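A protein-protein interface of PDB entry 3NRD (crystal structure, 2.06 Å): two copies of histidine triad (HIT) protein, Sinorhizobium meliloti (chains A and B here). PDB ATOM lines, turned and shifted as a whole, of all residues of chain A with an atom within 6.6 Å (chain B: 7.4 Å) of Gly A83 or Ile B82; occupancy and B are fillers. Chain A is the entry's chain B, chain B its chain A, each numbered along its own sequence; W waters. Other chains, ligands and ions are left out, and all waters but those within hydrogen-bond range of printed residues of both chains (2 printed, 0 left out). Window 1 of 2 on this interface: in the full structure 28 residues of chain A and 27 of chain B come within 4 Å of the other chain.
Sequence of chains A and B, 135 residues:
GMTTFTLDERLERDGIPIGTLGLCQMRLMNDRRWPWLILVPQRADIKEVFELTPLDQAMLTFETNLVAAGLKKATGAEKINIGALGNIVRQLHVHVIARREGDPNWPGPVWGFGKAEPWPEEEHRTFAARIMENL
NZ of Lys B79 is in salt-bridge range of OE1 of Glu A48, at 2.8 Å.
The backbone carbonyl oxygen (O) of Leu A85 lies within hydrogen-bond range of the side-chain amino group (NZ) of Lys B79.
The backbone NH (N) of Ile B80 sits at hydrogen-bond distance from the side-chain carboxylate (OE2) of Glu A48 (3.2 Å).
O of Leu A85 is in hydrogen-bond range of ND2 of Asn B81, at 3.0 Å.
The backbone carbonyl oxygen of Ile B82 sits at hydrogen-bond distance from the backbone NH of Ala A84, 2.8 Å away.
The backbone carbonyl oxygen (O) of Ile A82 sits at hydrogen-bond distance from the backbone NH (N) of Ala B84 (2.8 Å).
The backbone carbonyl oxygen of Leu B85 is in hydrogen-bond range of the side-chain amide nitrogen of Asn A81 (3.1 Å).
O of Ile B80 lies close to O of Leu A85, 3.3 Å away.
The backbone NH (N) of Ile B97 sits at hydrogen-bond distance from the backbone carbonyl oxygen (O) of Asn B81 (2.8 Å).
The backbone carbonyl oxygen of Gly B83 is in hydrogen-bond range of the backbone NH of His B95.
NE1 of Trp B111 sits close to ND1 of His B95, 3.5 Å away.
The backbone NH of Asn A81 lies within hydrogen-bond range of the backbone carbonyl oxygen of Ile A97 (2.8 Å).
The backbone carbonyl oxygen of Gly A83 lies within hydrogen-bond range of the backbone NH of His A95, 2.7 Å away.
NE1 of Trp A111 is in hydrogen-bond range of ND1 of His A95 (3.4 Å).
Among the printed residues, pairs that only touch across the chains: Val A49 with Asn B65, Val A49 with Ile B82, Phe A50 with Asn B65, Phe A50 with Ala B68, Phe A50 with Ala B69, Asn A81 with Ala B84, Ile A82 with Gly B83, Ile A82 with Leu B85, Gly A83 with Ile B82, Ala A84 with Asn B81, Leu A85 with Trp B111, Trp A111 with Leu B85 and Trp A111 with Trp B111.
Of chain B, only Ile B82 comes within 4 Å of Gly A83.
Of the printed residues of chain B, Trp A111 touches Leu B85 and Trp B111.
Of the printed residues of chain A, Ile B80 touches Glu A48 (3.2 Å) and Leu A85 (3.3 Å).
Of the printed residues of chain A, Ile B82 touches Val A49 (3.6 Å), Gly A83 (3.4 Å) and Ala A84 (2.8 Å).
Printed residues of chain A within 4 Å of Ala B84: Asn A81 (3.5 Å) and Ile A82 (2.8 Å).
Of the printed residues of chain A, Leu B85 touches Asn A81 (3.1 Å), Ile A82 (3.8 Å) and Trp A111 (3.8 Å).
The nearest residue of chain B that does not touch Gly A83 is Gly B83 (4.3 Å).
The nearest printed residue of chain A that does not touch Ile B82 is Leu A85 (4.01 Å).
The nearest printed residue of chain B that does not touch Ile A82 is Ile B82 (4.2 Å).
Printed residues of chain A that touch a printed residue of chain B: Glu A48, Val A49, Phe A50, Asn A81, Ile A82, Gly A83, Ala A84, Leu A85 and Trp A111.
Of the 17 printed residues of chain B, 11 touch a printed residue of chain A.
Among the printed residues, 21 pairs touch across the chains.
Among the printed residues, Asp or Glu carboxylates within 4 Å of a Lys or Arg side-chain nitrogen of the other chain: Glu A48 with Lys B79 (2.8 Å).
Asn A81 touches Ala B84, and with the chains exchanged Ala A84 touches Asn B81.
Ile A82 touches Gly B83, and with the chains exchanged Gly A83 touches Ile B82.
Ile A82 touches Ala B84, and with the chains exchanged Ala A84 touches Ile B82.
Leu A85 touches Trp B111, and with the chains exchanged Trp A111 touches Leu B85.
10 positions are printed for both chains.
Water W1 lies within hydrogen-bond range of NZ of Lys B79 (2.6 Å), O of Ala A84 (3.4 Å) and O of Leu A85 (3.5 Å).
Water W2 lies within hydrogen-bond range of O of Ala A84 (2.7 Å), O of Ile B80 (2.8 Å) and N of Ile B82 (3.4 Å).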
ATOM      1  N   GLU A  48       6.342 -23.164 -36.399  1.00  0.00           N
ATOM      2  CA  GLU A  48       7.741 -22.755 -36.190  1.00  0.00           C
ATOM      3  C   GLU A  48       7.791 -21.306 -35.791  1.00  0.00           C
ATOM      4  O   GLU A  48       6.975 -20.495 -36.263  1.00  0.00           O
ATOM      5  CB  GLU A  48       8.544 -22.937 -37.468  1.00  0.00           C
ATOM      6  CG  GLU A  48       8.509 -24.323 -38.074  1.00  0.00           C
ATOM      7  CD  GLU A  48       9.399 -25.357 -37.371  1.00  0.00           C
ATOM      8  OE1 GLU A  48       9.851 -25.184 -36.204  1.00  0.00           O
ATOM      9  OE2 GLU A  48       9.622 -26.388 -38.027  1.00  0.00           O
ATOM     10  N   VAL A  49       8.790 -20.954 -34.990  1.00  0.00           N
ATOM     11  CA  VAL A  49       8.995 -19.580 -34.570  1.00  0.00           C
ATOM     12  C   VAL A  49       9.056 -18.631 -35.801  1.00  0.00           C
ATOM     13  O   VAL A  49       8.459 -17.564 -35.822  1.00  0.00           O
ATOM     14  CB  VAL A  49      10.248 -19.498 -33.640  1.00  0.00           C
ATOM     15  CG1 VAL A  49      11.554 -19.523 -34.459  1.00  0.00           C
ATOM     16  CG2 VAL A  49      10.161 -18.294 -32.727  1.00  0.00           C
ATOM     17  N   PHE A  50       9.733 -19.060 -36.856  1.00  0.00           N
ATOM     18  CA  PHE A  50       9.925 -18.248 -38.067  1.00  0.00           C
ATOM     19  C   PHE A  50       8.710 -18.165 -38.999  1.00  0.00           C
ATOM     20  O   PHE A  50       8.776 -17.508 -40.021  1.00  0.00           O
ATOM     21  CB  PHE A  50      11.166 -18.712 -38.866  1.00  0.00           C
ATOM     22  CG  PHE A  50      11.159 -20.164 -39.236  1.00  0.00           C
ATOM     23  CD1 PHE A  50      10.501 -20.601 -40.363  1.00  0.00           C
ATOM     24  CD2 PHE A  50      11.821 -21.103 -38.431  1.00  0.00           C
ATOM     25  CE1 PHE A  50      10.506 -21.941 -40.714  1.00  0.00           C
ATOM     26  CE2 PHE A  50      11.831 -22.459 -38.776  1.00  0.00           C
ATOM     27  CZ  PHE A  50      11.167 -22.863 -39.919  1.00  0.00           C
ATOM     28  N   ASN A  81      15.784 -22.489 -18.316  1.00  0.00           N
ATOM     29  CA  ASN A  81      15.849 -23.198 -19.593  1.00  0.00           C
ATOM     30  C   ASN A  81      14.687 -22.782 -20.481  1.00  0.00           C
ATOM     31  O   ASN A  81      13.531 -22.762 -20.037  1.00  0.00           O
ATOM     32  CB  ASN A  81      15.795 -24.717 -19.410  1.00  0.00           C
ATOM     33  CG  ASN A  81      17.045 -25.304 -18.715  1.00  0.00           C
ATOM     34  OD1 ASN A  81      17.090 -26.519 -18.451  1.00  0.00           O
ATOM     35  ND2 ASN A  81      18.050 -24.474 -18.442  1.00  0.00           N
ATOM     36  N   ILE A  82      14.986 -22.476 -21.735  1.00  0.00           N
ATOM     37  CA  ILE A  82      13.975 -22.070 -22.686  1.00  0.00           C
ATOM     38  C   ILE A  82      14.063 -23.014 -23.865  1.00  0.00           C
ATOM     39  O   ILE A  82      15.159 -23.304 -24.340  1.00  0.00           O
ATOM     40  CB  ILE A  82      14.197 -20.644 -23.196  1.00  0.00           C
ATOM     41  CG1 ILE A  82      14.070 -19.612 -22.084  1.00  0.00           C
ATOM     42  CG2 ILE A  82      13.193 -20.302 -24.304  1.00  0.00           C
ATOM     43  CD1 ILE A  82      14.600 -18.231 -22.562  1.00  0.00           C
ATOM     44  N   GLY A  83      12.915 -23.510 -24.296  1.00  0.00           N
ATOM     45  CA  GLY A  83      12.832 -24.446 -25.398  1.00  0.00           C
ATOM     46  C   GLY A  83      11.574 -24.197 -26.207  1.00  0.00           C
ATOM     47  O   GLY A  83      10.458 -24.074 -25.650  1.00  0.00           O
ATOM     48  N   ALA A  84      11.743 -24.137 -27.518  1.00  0.00           N
ATOM     49  CA  ALA A  84      10.618 -24.239 -28.469  1.00  0.00           C
ATOM     50  C   ALA A  84      10.838 -25.479 -29.275  1.00  0.00           C
ATOM     51  O   ALA A  84      11.665 -25.473 -30.190  1.00  0.00           O
ATOM     52  CB  ALA A  84      10.550 -23.018 -29.367  1.00  0.00           C
ATOM     53  N   LEU A  85      10.136 -26.561 -28.912  1.00  0.00           N
ATOM     54  CA  LEU A  85      10.425 -27.876 -29.459  1.00  0.00           C
ATOM     55  C   LEU A  85       9.292 -28.228 -30.432  1.00  0.00           C
ATOM     56  O   LEU A  85       9.456 -28.101 -31.662  1.00  0.00           O
ATOM     57  CB  LEU A  85      10.654 -28.915 -28.325  1.00  0.00           C
ATOM     58  CG  LEU A  85      11.602 -28.560 -27.169  1.00  0.00           C
ATOM     59  CD1 LEU A  85      11.665 -29.738 -26.233  1.00  0.00           C
ATOM     60  CD2 LEU A  85      13.017 -28.164 -27.641  1.00  0.00           C
ATOM     61  N   HIS A  93       4.662 -23.181 -28.979  1.00  0.00           N
ATOM     62  CA  HIS A  93       4.662 -22.814 -27.584  1.00  0.00           C
ATOM     63  C   HIS A  93       6.074 -22.895 -27.077  1.00  0.00           C
ATOM     64  O   HIS A  93       6.838 -23.773 -27.504  1.00  0.00           O
ATOM     65  CB  HIS A  93       3.727 -23.700 -26.763  1.00  0.00           C
ATOM     66  CG  HIS A  93       4.057 -25.162 -26.794  1.00  0.00           C
ATOM     67  ND1 HIS A  93       3.946 -25.930 -27.934  1.00  0.00           N
ATOM     68  CD2 HIS A  93       4.421 -26.012 -25.798  1.00  0.00           C
ATOM     69  CE1 HIS A  93       4.260 -27.184 -27.646  1.00  0.00           C
ATOM     70  NE2 HIS A  93       4.567 -27.258 -26.360  1.00  0.00           N
ATOM     71  N   VAL A  94       6.414 -21.977 -26.187  1.00  0.00           N
ATOM     72  CA  VAL A  94       7.760 -21.858 -25.672  1.00  0.00           C
ATOM     73  C   VAL A  94       7.760 -22.276 -24.237  1.00  0.00           C
ATOM     74  O   VAL A  94       7.048 -21.691 -23.431  1.00  0.00           O
ATOM     75  CB  VAL A  94       8.293 -20.422 -25.738  1.00  0.00           C
ATOM     76  CG1 VAL A  94       9.683 -20.325 -25.073  1.00  0.00           C
ATOM     77  CG2 VAL A  94       8.342 -19.956 -27.178  1.00  0.00           C
ATOM     78  N   HIS A  95       8.601 -23.257 -23.916  1.00  0.00           N
ATOM     79  CA  HIS A  95       8.762 -23.725 -22.557  1.00  0.00           C
ATOM     80  C   HIS A  95       9.726 -22.804 -21.888  1.00  0.00           C
ATOM     81  O   HIS A  95      10.764 -22.508 -22.471  1.00  0.00           O
ATOM     82  CB  HIS A  95       9.369 -25.111 -22.529  1.00  0.00           C
ATOM     83  CG  HIS A  95       8.581 -26.147 -23.270  1.00  0.00           C
ATOM     84  ND1 HIS A  95       7.644 -26.934 -22.653  1.00  0.00           N
ATOM     85  CD2 HIS A  95       8.664 -26.590 -24.550  1.00  0.00           C
ATOM     86  CE1 HIS A  95       7.155 -27.799 -23.524  1.00  0.00           C
ATOM     87  NE2 HIS A  95       7.776 -27.627 -24.680  1.00  0.00           N
ATOM     88  N   VAL A  96       9.406 -22.361 -20.679  1.00  0.00           N
ATOM     89  CA  VAL A  96      10.285 -21.533 -19.862  1.00  0.00           C
ATOM     90  C   VAL A  96      10.313 -22.125 -18.472  1.00  0.00           C
ATOM     91  O   VAL A  96       9.306 -22.111 -17.793  1.00  0.00           O
ATOM     92  CB  VAL A  96       9.820 -20.078 -19.790  1.00  0.00           C
ATOM     93  CG1 VAL A  96      10.801 -19.261 -18.972  1.00  0.00           C
ATOM     94  CG2 VAL A  96       9.647 -19.487 -21.196  1.00  0.00           C
ATOM     95  N   ILE A  97      11.490 -22.620 -18.051  1.00  0.00           N
ATOM     96  CA  ILE A  97      11.612 -23.549 -16.947  1.00  0.00           C
ATOM     97  C   ILE A  97      12.705 -23.103 -15.954  1.00  0.00           C
ATOM     98  O   ILE A  97      13.844 -22.795 -16.354  1.00  0.00           O
ATOM     99  CB  ILE A  97      11.943 -24.959 -17.454  1.00  0.00           C
ATOM    100  CG1 ILE A  97      10.862 -25.506 -18.395  1.00  0.00           C
ATOM    101  CG2 ILE A  97      12.104 -25.931 -16.269  1.00  0.00           C
ATOM    102  CD1 ILE A  97      11.359 -26.569 -19.326  1.00  0.00           C
ATOM    103  N   TRP A 111      12.161 -32.477 -20.362  1.00  0.00           N
ATOM    104  CA  TRP A 111      11.281 -32.999 -21.381  1.00  0.00           C
ATOM    105  C   TRP A 111      11.505 -34.470 -21.512  1.00  0.00           C
ATOM    106  O   TRP A 111      12.632 -34.925 -21.655  1.00  0.00           O
ATOM    107  CB  TRP A 111      11.534 -32.327 -22.732  1.00  0.00           C
ATOM    108  CG  TRP A 111      11.323 -30.890 -22.667  1.00  0.00           C
ATOM    109  CD1 TRP A 111      10.151 -30.265 -22.457  1.00  0.00           C
ATOM    110  CD2 TRP A 111      12.323 -29.869 -22.746  1.00  0.00           C
ATOM    111  NE1 TRP A 111      10.341 -28.916 -22.444  1.00  0.00           N
ATOM    112  CE2 TRP A 111      11.666 -28.641 -22.599  1.00  0.00           C
ATOM    113  CE3 TRP A 111      13.707 -29.874 -22.928  1.00  0.00           C
ATOM    114  CZ2 TRP A 111      12.337 -27.415 -22.656  1.00  0.00           C
ATOM    115  CZ3 TRP A 111      14.373 -28.660 -22.984  1.00  0.00           C
ATOM    116  CH2 TRP A 111      13.688 -27.450 -22.842  1.00  0.00           C
ATOM    117  N   THR B  61      17.372 -13.066 -31.856  1.00  0.00           N
ATOM    118  CA  THR B  61      16.079 -13.594 -32.331  1.00  0.00           C
ATOM    119  C   THR B  61      16.134 -13.882 -33.809  1.00  0.00           C
ATOM    120  O   THR B  61      15.871 -14.987 -34.241  1.00  0.00           O
ATOM    121  CB  THR B  61      14.931 -12.586 -32.006  1.00  0.00           C
ATOM    122  OG1 THR B  61      14.839 -12.485 -30.585  1.00  0.00           O
ATOM    123  CG2 THR B  61      13.593 -13.017 -32.594  1.00  0.00           C
ATOM    124  N   THR B  64      18.778 -16.349 -34.897  1.00  0.00           N
ATOM    125  CA  THR B  64      18.281 -17.698 -34.560  1.00  0.00           C
ATOM    126  C   THR B  64      17.265 -18.198 -35.589  1.00  0.00           C
ATOM    127  O   THR B  64      17.371 -19.327 -36.061  1.00  0.00           O
ATOM    128  CB  THR B  64      17.688 -17.760 -33.157  1.00  0.00           C
ATOM    129  OG1 THR B  64      18.720 -17.528 -32.181  1.00  0.00           O
ATOM    130  CG2 THR B  64      17.068 -19.134 -32.883  1.00  0.00           C
ATOM    131  N   ASN B  65      16.353 -17.306 -35.969  1.00  0.00           N
ATOM    132  CA  ASN B  65      15.223 -17.618 -36.796  1.00  0.00           C
ATOM    133  C   ASN B  65      15.635 -17.746 -38.253  1.00  0.00           C
ATOM    134  O   ASN B  65      15.115 -18.625 -38.953  1.00  0.00           O
ATOM    135  CB  ASN B  65      14.091 -16.592 -36.577  1.00  0.00           C
ATOM    136  CG  ASN B  65      13.472 -16.701 -35.159  1.00  0.00           C
ATOM    137  OD1 ASN B  65      13.793 -17.626 -34.419  1.00  0.00           O
ATOM    138  ND2 ASN B  65      12.633 -15.742 -34.780  1.00  0.00           N
ATOM    139  N   ALA B  68      17.301 -21.102 -38.238  1.00  0.00           N
ATOM    140  CA  ALA B  68      16.291 -22.165 -38.113  1.00  0.00           C
ATOM    141  C   ALA B  68      15.627 -22.423 -39.481  1.00  0.00           C
ATOM    142  O   ALA B  68      15.511 -23.560 -39.902  1.00  0.00           O
ATOM    143  CB  ALA B  68      15.252 -21.803 -37.069  1.00  0.00           C
ATOM    144  N   ALA B  69      15.208 -21.348 -40.147  1.00  0.00           N
ATOM    145  CA  ALA B  69      14.614 -21.446 -41.504  1.00  0.00           C
ATOM    146  C   ALA B  69      15.620 -22.052 -42.471  1.00  0.00           C
ATOM    147  O   ALA B  69      15.288 -22.963 -43.218  1.00  0.00           O
ATOM    148  CB  ALA B  69      14.131 -20.069 -41.988  1.00  0.00           C
ATOM    149  N   LYS B  79      10.610 -30.548 -38.428  1.00  0.00           N
ATOM    150  CA  LYS B  79      10.486 -29.633 -37.306  1.00  0.00           C
ATOM    151  C   LYS B  79      11.844 -29.185 -36.794  1.00  0.00           C
ATOM    152  O   LYS B  79      12.776 -29.998 -36.670  1.00  0.00           O
ATOM    153  CB  LYS B  79       9.708 -30.303 -36.173  1.00  0.00           C
ATOM    154  CG  LYS B  79       9.261 -29.387 -35.035  1.00  0.00           C
ATOM    155  CD  LYS B  79       8.145 -28.427 -35.460  1.00  0.00           C
ATOM    156  CE  LYS B  79       7.779 -27.469 -34.325  1.00  0.00           C
ATOM    157  NZ  LYS B  79       8.861 -26.523 -34.009  1.00  0.00           N
ATOM    158  N   ILE B  80      11.961 -27.898 -36.506  1.00  0.00           N
ATOM    159  CA  ILE B  80      13.107 -27.363 -35.804  1.00  0.00           C
ATOM    160  C   ILE B  80      12.823 -27.312 -34.298  1.00  0.00           C
ATOM    161  O   ILE B  80      11.695 -26.999 -33.894  1.00  0.00           O
ATOM    162  CB  ILE B  80      13.464 -25.942 -36.301  1.00  0.00           C
ATOM    163  CG1 ILE B  80      13.857 -25.955 -37.794  1.00  0.00           C
ATOM    164  CG2 ILE B  80      14.625 -25.331 -35.504  1.00  0.00           C
ATOM    165  CD1 ILE B  80      15.153 -26.725 -38.106  1.00  0.00           C
ATOM    166  N   ASN B  81      13.844 -27.629 -33.488  1.00  0.00           N
ATOM    167  CA  ASN B  81      13.834 -27.451 -32.045  1.00  0.00           C
ATOM    168  C   ASN B  81      14.880 -26.389 -31.709  1.00  0.00           C
ATOM    169  O   ASN B  81      15.996 -26.490 -32.179  1.00  0.00           O
ATOM    170  CB  ASN B  81      14.196 -28.729 -31.293  1.00  0.00           C
ATOM    171  CG  ASN B  81      13.178 -29.857 -31.454  1.00  0.00           C
ATOM    172  OD1 ASN B  81      13.462 -30.971 -31.054  1.00  0.00           O
ATOM    173  ND2 ASN B  81      12.008 -29.577 -32.028  1.00  0.00           N
ATOM    174  N   ILE B  82      14.498 -25.383 -30.927  1.00  0.00           N
ATOM    175  CA  ILE B  82      15.374 -24.297 -30.513  1.00  0.00           C
ATOM    176  C   ILE B  82      15.475 -24.346 -29.018  1.00  0.00           C
ATOM    177  O   ILE B  82      14.445 -24.489 -28.351  1.00  0.00           O
ATOM    178  CB  ILE B  82      14.811 -22.940 -30.929  1.00  0.00           C
ATOM    179  CG1 ILE B  82      14.872 -22.806 -32.460  1.00  0.00           C
ATOM    180  CG2 ILE B  82      15.599 -21.825 -30.254  1.00  0.00           C
ATOM    181  CD1 ILE B  82      14.037 -21.707 -33.007  1.00  0.00           C
ATOM    182  N   GLY B  83      16.670 -24.168 -28.465  1.00  0.00           N
ATOM    183  CA  GLY B  83      16.853 -24.339 -27.009  1.00  0.00           C
ATOM    184  C   GLY B  83      17.971 -23.509 -26.446  1.00  0.00           C
ATOM    185  O   GLY B  83      19.015 -23.402 -27.066  1.00  0.00           O
ATOM    186  N   ALA B  84      17.727 -22.875 -25.297  1.00  0.00           N
ATOM    187  CA  ALA B  84      18.751 -22.122 -24.539  1.00  0.00           C
ATOM    188  C   ALA B  84      18.640 -22.734 -23.182  1.00  0.00           C
ATOM    189  O   ALA B  84      17.657 -22.470 -22.505  1.00  0.00           O
ATOM    190  CB  ALA B  84      18.462 -20.617 -24.498  1.00  0.00           C
ATOM    191  N   LEU B  85      19.586 -23.597 -22.819  1.00  0.00           N
ATOM    192  CA  LEU B  85      19.533 -24.366 -21.595  1.00  0.00           C
ATOM    193  C   LEU B  85      20.640 -23.863 -20.678  1.00  0.00           C
ATOM    194  O   LEU B  85      20.384 -23.038 -19.817  1.00  0.00           O
ATOM    195  CB  LEU B  85      19.599 -25.889 -21.888  1.00  0.00           C
ATOM    196  CG  LEU B  85      18.640 -26.406 -22.994  1.00  0.00           C
ATOM    197  CD1 LEU B  85      18.787 -27.925 -23.220  1.00  0.00           C
ATOM    198  CD2 LEU B  85      17.221 -26.066 -22.676  1.00  0.00           C
ATOM    199  N   VAL B  94      22.574 -20.960 -28.111  1.00  0.00           N
ATOM    200  CA  VAL B  94      21.230 -21.344 -28.512  1.00  0.00           C
ATOM    201  C   VAL B  94      21.377 -22.499 -29.457  1.00  0.00           C
ATOM    202  O   VAL B  94      22.039 -22.352 -30.509  1.00  0.00           O
ATOM    203  CB  VAL B  94      20.476 -20.222 -29.194  1.00  0.00           C
ATOM    204  CG1 VAL B  94      19.100 -20.720 -29.647  1.00  0.00           C
ATOM    205  CG2 VAL B  94      20.337 -19.009 -28.255  1.00  0.00           C
ATOM    206  N   HIS B  95      20.786 -23.633 -29.079  1.00  0.00           N
ATOM    207  CA  HIS B  95      20.703 -24.822 -29.898  1.00  0.00           C
ATOM    208  C   HIS B  95      19.627 -24.623 -30.960  1.00  0.00           C
ATOM    209  O   HIS B  95      18.546 -24.139 -30.641  1.00  0.00           O
ATOM    210  CB  HIS B  95      20.327 -26.054 -29.055  1.00  0.00           C
ATOM    211  CG  HIS B  95      21.222 -26.308 -27.871  1.00  0.00           C
ATOM    212  ND1 HIS B  95      22.393 -27.022 -27.960  1.00  0.00           N
ATOM    213  CD2 HIS B  95      21.077 -25.995 -26.561  1.00  0.00           C
ATOM    214  CE1 HIS B  95      22.955 -27.108 -26.764  1.00  0.00           C
ATOM    215  NE2 HIS B  95      22.164 -26.512 -25.888  1.00  0.00           N
ATOM    216  N   VAL B  96      19.919 -25.004 -32.208  1.00  0.00           N
ATOM    217  CA  VAL B  96      18.975 -24.978 -33.320  1.00  0.00           C
ATOM    218  C   VAL B  96      19.141 -26.296 -34.036  1.00  0.00           C
ATOM    219  O   VAL B  96      20.155 -26.525 -34.698  1.00  0.00           O
ATOM    220  CB  VAL B  96      19.249 -23.836 -34.298  1.00  0.00           C
ATOM    221  CG1 VAL B  96      18.177 -23.823 -35.438  1.00  0.00           C
ATOM    222  CG2 VAL B  96      19.311 -22.510 -33.568  1.00  0.00           C
ATOM    223  N   ILE B  97      18.158 -27.170 -33.869  1.00  0.00           N
ATOM    224  CA  ILE B  97      18.306 -28.585 -34.184  1.00  0.00           C
ATOM    225  C   ILE B  97      17.222 -29.004 -35.183  1.00  0.00           C
ATOM    226  O   ILE B  97      16.052 -28.687 -34.976  1.00  0.00           O
ATOM    227  CB  ILE B  97      18.148 -29.461 -32.954  1.00  0.00           C
ATOM    228  CG1 ILE B  97      19.142 -29.079 -31.830  1.00  0.00           C
ATOM    229  CG2 ILE B  97      18.329 -30.923 -33.343  1.00  0.00           C
ATOM    230  CD1 ILE B  97      18.582 -29.252 -30.454  1.00  0.00           C
ATOM    231  N   TRP B 111      18.995 -33.595 -26.152  1.00  0.00           N
ATOM    232  CA  TRP B 111      19.878 -33.287 -25.029  1.00  0.00           C
ATOM    233  C   TRP B 111      19.901 -34.431 -24.044  1.00  0.00           C
ATOM    234  O   TRP B 111      18.854 -34.894 -23.579  1.00  0.00           O
ATOM    235  CB  TRP B 111      19.419 -31.995 -24.338  1.00  0.00           C
ATOM    236  CG  TRP B 111      19.385 -30.832 -25.291  1.00  0.00           C
ATOM    237  CD1 TRP B 111      20.457 -30.240 -25.868  1.00  0.00           C
ATOM    238  CD2 TRP B 111      18.231 -30.168 -25.801  1.00  0.00           C
ATOM    239  NE1 TRP B 111      20.054 -29.247 -26.717  1.00  0.00           N
ATOM    240  CE2 TRP B 111      18.689 -29.171 -26.695  1.00  0.00           C
ATOM    241  CE3 TRP B 111      16.857 -30.298 -25.582  1.00  0.00           C
ATOM    242  CZ2 TRP B 111      17.824 -28.303 -27.355  1.00  0.00           C
ATOM    243  CZ3 TRP B 111      15.997 -29.454 -26.267  1.00  0.00           C
ATOM    244  CH2 TRP B 111      16.483 -28.464 -27.136  1.00  0.00           C
HETATM  245  O   HOH W   1       8.932 -24.711 -32.112  1.00  0.00           O
HETATM  246  O   HOH W   2      11.736 -24.473 -32.669  1.00  0.00           O
